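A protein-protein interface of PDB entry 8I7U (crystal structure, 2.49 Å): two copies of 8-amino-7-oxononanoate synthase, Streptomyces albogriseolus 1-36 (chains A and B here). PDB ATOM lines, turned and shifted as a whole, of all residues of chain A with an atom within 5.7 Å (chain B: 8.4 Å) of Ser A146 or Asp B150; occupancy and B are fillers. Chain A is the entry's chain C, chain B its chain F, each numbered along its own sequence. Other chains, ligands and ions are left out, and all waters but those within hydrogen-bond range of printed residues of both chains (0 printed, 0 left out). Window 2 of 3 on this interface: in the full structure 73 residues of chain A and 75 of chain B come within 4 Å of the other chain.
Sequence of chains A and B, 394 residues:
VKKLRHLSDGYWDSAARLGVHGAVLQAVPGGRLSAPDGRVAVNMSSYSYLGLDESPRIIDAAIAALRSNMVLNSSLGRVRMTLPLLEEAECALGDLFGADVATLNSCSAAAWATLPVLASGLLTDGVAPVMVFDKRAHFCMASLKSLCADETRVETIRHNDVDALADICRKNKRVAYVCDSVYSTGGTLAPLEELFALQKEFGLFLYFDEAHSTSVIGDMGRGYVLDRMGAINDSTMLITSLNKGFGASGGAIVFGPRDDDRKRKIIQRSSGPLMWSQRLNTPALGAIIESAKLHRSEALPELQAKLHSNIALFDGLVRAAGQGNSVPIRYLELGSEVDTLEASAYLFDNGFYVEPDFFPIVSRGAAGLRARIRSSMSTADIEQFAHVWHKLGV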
ATOM      1  N   ALA A 142     -24.393 -21.540   5.856  1.00  0.00           N
ATOM      2  CA  ALA A 142     -24.415 -21.611   7.313  1.00  0.00           C
ATOM      3  C   ALA A 142     -23.236 -20.876   7.937  1.00  0.00           C
ATOM      4  O   ALA A 142     -23.340 -20.395   9.067  1.00  0.00           O
ATOM      5  CB  ALA A 142     -24.440 -23.071   7.766  1.00  0.00           C
ATOM      6  N   SER A 143     -22.112 -20.771   7.229  1.00  0.00           N
ATOM      7  CA  SER A 143     -20.996 -19.986   7.741  1.00  0.00           C
ATOM      8  C   SER A 143     -21.280 -18.481   7.771  1.00  0.00           C
ATOM      9  O   SER A 143     -20.433 -17.724   8.260  1.00  0.00           O
ATOM     10  CB  SER A 143     -19.759 -20.230   6.897  1.00  0.00           C
ATOM     11  OG  SER A 143     -19.750 -19.303   5.826  1.00  0.00           O
ATOM     12  N   LEU A 144     -22.428 -18.031   7.257  1.00  0.00           N
ATOM     13  CA  LEU A 144     -22.792 -16.619   7.222  1.00  0.00           C
ATOM     14  C   LEU A 144     -23.872 -16.267   8.241  1.00  0.00           C
ATOM     15  O   LEU A 144     -24.434 -15.164   8.178  1.00  0.00           O
ATOM     16  CB  LEU A 144     -23.268 -16.224   5.820  1.00  0.00           C
ATOM     17  CG  LEU A 144     -22.282 -16.467   4.686  1.00  0.00           C
ATOM     18  CD1 LEU A 144     -22.897 -16.122   3.360  1.00  0.00           C
ATOM     19  CD2 LEU A 144     -20.997 -15.682   4.911  1.00  0.00           C
ATOM     20  N   LYS A 145     -24.195 -17.188   9.159  1.00  0.00           N
ATOM     21  CA  LYS A 145     -25.184 -16.897  10.192  1.00  0.00           C
ATOM     22  C   LYS A 145     -24.855 -15.622  10.958  1.00  0.00           C
ATOM     23  O   LYS A 145     -25.764 -14.873  11.337  1.00  0.00           O
ATOM     24  CB  LYS A 145     -25.289 -18.078  11.146  1.00  0.00           C
ATOM     25  CG  LYS A 145     -25.833 -19.319  10.493  1.00  0.00           C
ATOM     26  CD  LYS A 145     -25.812 -20.479  11.463  1.00  0.00           C
ATOM     27  CE  LYS A 145     -26.274 -21.745  10.815  1.00  0.00           C
ATOM     28  NZ  LYS A 145     -26.496 -22.712  11.896  1.00  0.00           N
ATOM     29  N   SER A 146     -23.567 -15.346  11.178  1.00  0.00           N
ATOM     30  CA  SER A 146     -23.190 -14.203  11.995  1.00  0.00           C
ATOM     31  C   SER A 146     -23.449 -12.883  11.285  1.00  0.00           C
ATOM     32  O   SER A 146     -23.757 -11.887  11.948  1.00  0.00           O
ATOM     33  CB  SER A 146     -21.731 -14.307  12.414  1.00  0.00           C
ATOM     34  OG  SER A 146     -21.619 -15.171  13.533  1.00  0.00           O
ATOM     35  N   LEU A 147     -23.330 -12.841   9.955  1.00  0.00           N
ATOM     36  CA  LEU A 147     -23.774 -11.646   9.243  1.00  0.00           C
ATOM     37  C   LEU A 147     -25.283 -11.503   9.336  1.00  0.00           C
ATOM     38  O   LEU A 147     -25.802 -10.387   9.464  1.00  0.00           O
ATOM     39  CB  LEU A 147     -23.350 -11.676   7.776  1.00  0.00           C
ATOM     40  CG  LEU A 147     -21.872 -11.687   7.438  1.00  0.00           C
ATOM     41  CD1 LEU A 147     -21.475 -13.118   7.295  1.00  0.00           C
ATOM     42  CD2 LEU A 147     -21.656 -10.956   6.144  1.00  0.00           C
ATOM     43  N   CYS A 148     -26.007 -12.624   9.279  1.00  0.00           N
ATOM     44  CA  CYS A 148     -27.453 -12.546   9.430  1.00  0.00           C
ATOM     45  C   CYS A 148     -27.822 -12.095  10.837  1.00  0.00           C
ATOM     46  O   CYS A 148     -28.758 -11.307  11.016  1.00  0.00           O
ATOM     47  CB  CYS A 148     -28.088 -13.898   9.094  1.00  0.00           C
ATOM     48  SG  CYS A 148     -27.753 -14.465   7.401  1.00  0.00           S
ATOM     49  N   ALA A 149     -27.073 -12.564  11.842  1.00  0.00           N
ATOM     50  CA  ALA A 149     -27.368 -12.219  13.226  1.00  0.00           C
ATOM     51  C   ALA A 149     -27.283 -10.723  13.453  1.00  0.00           C
ATOM     52  O   ALA A 149     -27.995 -10.183  14.304  1.00  0.00           O
ATOM     53  CB  ALA A 149     -26.412 -12.949  14.161  1.00  0.00           C
ATOM     54  N   ASP A 150     -26.427 -10.040  12.694  1.00  0.00           N
ATOM     55  CA  ASP A 150     -26.336  -8.588  12.730  1.00  0.00           C
ATOM     56  C   ASP A 150     -27.596  -7.905  12.238  1.00  0.00           C
ATOM     57  O   ASP A 150     -27.728  -6.693  12.423  1.00  0.00           O
ATOM     58  CB  ASP A 150     -25.157  -8.117  11.883  1.00  0.00           C
ATOM     59  CG  ASP A 150     -23.836  -8.446  12.506  1.00  0.00           C
ATOM     60  OD1 ASP A 150     -23.831  -8.885  13.675  1.00  0.00           O
ATOM     61  OD2 ASP A 150     -22.803  -8.268  11.823  1.00  0.00           O
ATOM     62  N   PRO B 116     -11.402 -15.626   8.743  1.00  0.00           N
ATOM     63  CA  PRO B 116     -11.873 -16.406   9.899  1.00  0.00           C
ATOM     64  C   PRO B 116     -10.786 -17.247  10.539  1.00  0.00           C
ATOM     65  O   PRO B 116     -10.688 -17.290  11.769  1.00  0.00           O
ATOM     66  CB  PRO B 116     -12.987 -17.266   9.302  1.00  0.00           C
ATOM     67  CG  PRO B 116     -13.548 -16.415   8.238  1.00  0.00           C
ATOM     68  CD  PRO B 116     -12.355 -15.724   7.618  1.00  0.00           C
ATOM     69  N   ALA B 119      -8.450 -15.124  12.520  1.00  0.00           N
ATOM     70  CA  ALA B 119      -9.086 -14.735  13.769  1.00  0.00           C
ATOM     71  C   ALA B 119      -8.974 -15.837  14.811  1.00  0.00           C
ATOM     72  O   ALA B 119      -8.838 -15.553  16.004  1.00  0.00           O
ATOM     73  CB  ALA B 119     -10.550 -14.381  13.507  1.00  0.00           C
ATOM     74  N   SER B 120      -9.001 -17.096  14.377  1.00  0.00           N
ATOM     75  CA  SER B 120      -8.996 -18.239  15.274  1.00  0.00           C
ATOM     76  C   SER B 120      -7.649 -18.492  15.947  1.00  0.00           C
ATOM     77  O   SER B 120      -7.592 -19.297  16.878  1.00  0.00           O
ATOM     78  CB  SER B 120      -9.405 -19.489  14.501  1.00  0.00           C
ATOM     79  OG  SER B 120      -8.330 -19.928  13.682  1.00  0.00           O
ATOM     80  N   ALA B 128      -5.306 -16.784  19.490  1.00  0.00           N
ATOM     81  CA  ALA B 128      -6.245 -15.907  18.801  1.00  0.00           C
ATOM     82  C   ALA B 128      -5.792 -14.458  18.924  1.00  0.00           C
ATOM     83  O   ALA B 128      -5.788 -13.901  20.032  1.00  0.00           O
ATOM     84  CB  ALA B 128      -7.659 -16.051  19.359  1.00  0.00           C
ATOM     85  N   SER B 143     -16.836  -6.715   5.788  1.00  0.00           N
ATOM     86  CA  SER B 143     -18.125  -7.370   6.012  1.00  0.00           C
ATOM     87  C   SER B 143     -17.984  -8.734   6.677  1.00  0.00           C
ATOM     88  O   SER B 143     -18.998  -9.392   6.932  1.00  0.00           O
ATOM     89  CB  SER B 143     -18.887  -7.510   4.693  1.00  0.00           C
ATOM     90  OG  SER B 143     -18.207  -8.375   3.796  1.00  0.00           O
ATOM     91  N   LEU B 144     -16.763  -9.172   6.967  1.00  0.00           N
ATOM     92  CA  LEU B 144     -16.519 -10.456   7.607  1.00  0.00           C
ATOM     93  C   LEU B 144     -16.157 -10.314   9.078  1.00  0.00           C
ATOM     94  O   LEU B 144     -15.758 -11.297   9.704  1.00  0.00           O
ATOM     95  CB  LEU B 144     -15.418 -11.205   6.859  1.00  0.00           C
ATOM     96  CG  LEU B 144     -15.806 -11.573   5.423  1.00  0.00           C
ATOM     97  CD1 LEU B 144     -14.781 -12.517   4.792  1.00  0.00           C
ATOM     98  CD2 LEU B 144     -17.213 -12.183   5.384  1.00  0.00           C
ATOM     99  N   LYS B 145     -16.298  -9.114   9.651  1.00  0.00           N
ATOM    100  CA  LYS B 145     -15.905  -8.914  11.041  1.00  0.00           C
ATOM    101  C   LYS B 145     -16.693  -9.825  11.975  1.00  0.00           C
ATOM    102  O   LYS B 145     -16.124 -10.431  12.893  1.00  0.00           O
ATOM    103  CB  LYS B 145     -16.095  -7.455  11.433  1.00  0.00           C
ATOM    104  CG  LYS B 145     -15.159  -6.487  10.750  1.00  0.00           C
ATOM    105  CD  LYS B 145     -15.480  -5.056  11.165  1.00  0.00           C
ATOM    106  CE  LYS B 145     -14.704  -4.052  10.327  1.00  0.00           C
ATOM    107  NZ  LYS B 145     -15.329  -2.691  10.397  1.00  0.00           N
ATOM    108  N   SER B 146     -18.000  -9.954  11.739  1.00  0.00           N
ATOM    109  CA  SER B 146     -18.833 -10.778  12.606  1.00  0.00           C
ATOM    110  C   SER B 146     -18.323 -12.212  12.688  1.00  0.00           C
ATOM    111  O   SER B 146     -18.405 -12.836  13.752  1.00  0.00           O
ATOM    112  CB  SER B 146     -20.280 -10.753  12.121  1.00  0.00           C
ATOM    113  OG  SER B 146     -20.850  -9.475  12.326  1.00  0.00           O
ATOM    114  N   LEU B 147     -17.813 -12.764  11.579  1.00  0.00           N
ATOM    115  CA  LEU B 147     -17.237 -14.107  11.637  1.00  0.00           C
ATOM    116  C   LEU B 147     -15.954 -14.098  12.446  1.00  0.00           C
ATOM    117  O   LEU B 147     -15.667 -15.043  13.187  1.00  0.00           O
ATOM    118  CB  LEU B 147     -16.947 -14.660  10.243  1.00  0.00           C
ATOM    119  CG  LEU B 147     -18.034 -14.854   9.196  1.00  0.00           C
ATOM    120  CD1 LEU B 147     -18.361 -13.525   8.587  1.00  0.00           C
ATOM    121  CD2 LEU B 147     -17.550 -15.827   8.119  1.00  0.00           C
ATOM    122  N   CYS B 148     -15.170 -13.028  12.315  1.00  0.00           N
ATOM    123  CA  CYS B 148     -13.994 -12.872  13.153  1.00  0.00           C
ATOM    124  C   CYS B 148     -14.396 -12.699  14.616  1.00  0.00           C
ATOM    125  O   CYS B 148     -13.806 -13.329  15.502  1.00  0.00           O
ATOM    126  CB  CYS B 148     -13.154 -11.695  12.643  1.00  0.00           C
ATOM    127  SG  CYS B 148     -12.509 -11.929  10.930  1.00  0.00           S
ATOM    128  N   ALA B 149     -15.444 -11.903  14.877  1.00  0.00           N
ATOM    129  CA  ALA B 149     -15.950 -11.702  16.235  1.00  0.00           C
ATOM    130  C   ALA B 149     -16.365 -13.003  16.927  1.00  0.00           C
ATOM    131  O   ALA B 149     -16.415 -13.043  18.160  1.00  0.00           O
ATOM    132  CB  ALA B 149     -17.136 -10.736  16.224  1.00  0.00           C
ATOM    133  N   ASP B 150     -16.680 -14.058  16.173  1.00  0.00           N
ATOM    134  CA  ASP B 150     -16.983 -15.355  16.768  1.00  0.00           C
ATOM    135  C   ASP B 150     -15.737 -16.092  17.216  1.00  0.00           C
ATOM    136  O   ASP B 150     -15.845 -17.211  17.732  1.00  0.00           O
ATOM    137  CB  ASP B 150     -17.741 -16.239  15.778  1.00  0.00           C
ATOM    138  CG  ASP B 150     -19.157 -15.781  15.553  1.00  0.00           C
ATOM    139  OD1 ASP B 150     -19.650 -14.952  16.349  1.00  0.00           O
ATOM    140  OD2 ASP B 150     -19.775 -16.245  14.567  1.00  0.00           O
ATOM    141  N   GLU B 151     -14.562 -15.510  17.008  1.00  0.00           N
ATOM    142  CA  GLU B 151     -13.317 -16.180  17.323  1.00  0.00           C
ATOM    143  C   GLU B 151     -12.425 -15.401  18.266  1.00  0.00           C
ATOM    144  O   GLU B 151     -11.556 -16.009  18.897  1.00  0.00           O
ATOM    145  CB  GLU B 151     -12.535 -16.471  16.033  1.00  0.00           C
ATOM    146  CG  GLU B 151     -13.328 -17.293  15.013  1.00  0.00           C
ATOM    147  CD  GLU B 151     -13.305 -18.785  15.313  1.00  0.00           C
ATOM    148  OE1 GLU B 151     -12.319 -19.254  15.922  1.00  0.00           O
ATOM    149  OE2 GLU B 151     -14.269 -19.488  14.947  1.00  0.00           O
ATOM    150  N   THR B 152     -12.621 -14.096  18.402  1.00  0.00           N
ATOM    151  CA  THR B 152     -11.684 -13.257  19.139  1.00  0.00           C
ATOM    152  C   THR B 152     -12.254 -11.844  19.163  1.00  0.00           C
ATOM    153  O   THR B 152     -13.334 -11.591  18.628  1.00  0.00           O
ATOM    154  CB  THR B 152     -10.295 -13.316  18.492  1.00  0.00           C
ATOM    155  OG1 THR B 152      -9.342 -12.671  19.334  1.00  0.00           O
ATOM    156  CG2 THR B 152     -10.310 -12.641  17.114  1.00  0.00           C
ATOM    157  N   ARG B 153     -11.541 -10.931  19.812  1.00  0.00           N
ATOM    158  CA  ARG B 153     -11.944  -9.533  19.828  1.00  0.00           C
ATOM    159  C   ARG B 153     -11.633  -8.873  18.487  1.00  0.00           C
ATOM    160  O   ARG B 153     -10.544  -9.038  17.928  1.00  0.00           O
ATOM    161  CB  ARG B 153     -11.218  -8.757  20.928  1.00  0.00           C
ATOM    162  CG  ARG B 153     -11.285  -9.365  22.293  1.00  0.00           C
ATOM    163  CD  ARG B 153     -10.100  -8.925  23.153  1.00  0.00           C
ATOM    164  NE  ARG B 153      -9.823  -7.505  22.980  1.00  0.00           N
ATOM    165  CZ  ARG B 153      -8.865  -6.840  23.614  1.00  0.00           C
ATOM    166  NH1 ARG B 153      -8.063  -7.433  24.489  1.00  0.00           N
ATOM    167  NH2 ARG B 153      -8.701  -5.545  23.355  1.00  0.00           N
ATOM    168  N   VAL B 154     -12.594  -8.103  17.985  1.00  0.00           N
ATOM    169  CA  VAL B 154     -12.457  -7.329  16.756  1.00  0.00           C
ATOM    170  C   VAL B 154     -12.464  -5.855  17.134  1.00  0.00           C
ATOM    171  O   VAL B 154     -13.301  -5.422  17.936  1.00  0.00           O
ATOM    172  CB  VAL B 154     -13.590  -7.648  15.765  1.00  0.00           C
ATOM    173  CG1 VAL B 154     -13.570  -6.705  14.577  1.00  0.00           C
ATOM    174  CG2 VAL B 154     -13.494  -9.079  15.320  1.00  0.00           C
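OD1 of Asp A150 sits close to OG of Ser B146, at 3.3 Å. The side-chain carboxylate (OD1) of Asp B150 lies close to the side-chain hydroxyl (OG) of Ser A146 (3.4 Å).
Ser A143 touches Leu B147, and with the chains exchanged Leu A147 touches Ser B143. Ser A146 touches its own counterpart, Ser B146. Ser A146 touches Asp B150, and with the chains exchanged Asp A150 touches Ser B146. Leu B147 touches its own counterpart, Leu A147. Positions printed for both chains: 143, 144, 145, 146, 147, 148, 149 and 150.
Hydrophobic or aromatic side chains of chain A that line the printed part of chain B: Leu A147. Of the 16 printed residues of chain B, 4 touch a printed residue of chain A.
Leu B147 touches Ser A143. Ser A146 touches Ser B146 (O to CB, 3.7 Å). Leu A147 touches Ser B143. Leu A147 touches Leu B147 (CD1 to CD1, 3.4 Å).
Of chain B, only Ser B146 (3.7 Å) and Asp B150 (2.4 Å) come within 4 Å of Ser A146. Of the printed residues of chain A, Asp B150 touches Ser A146 (2.4 Å). Of the printed residues of chain B, Asp A150 touches Ser B146. Of the printed residues of chain B, Ser A143 touches Leu B147 (3.5 Å). Pro B116 touches none of the printed residues of chain A. The nearest residue of chain B that does not touch Ser A146 is Leu B147 (4.3 Å). The nearest printed residue of chain A that does not touch Ser B143 is Asp A150 (6.3 Å).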
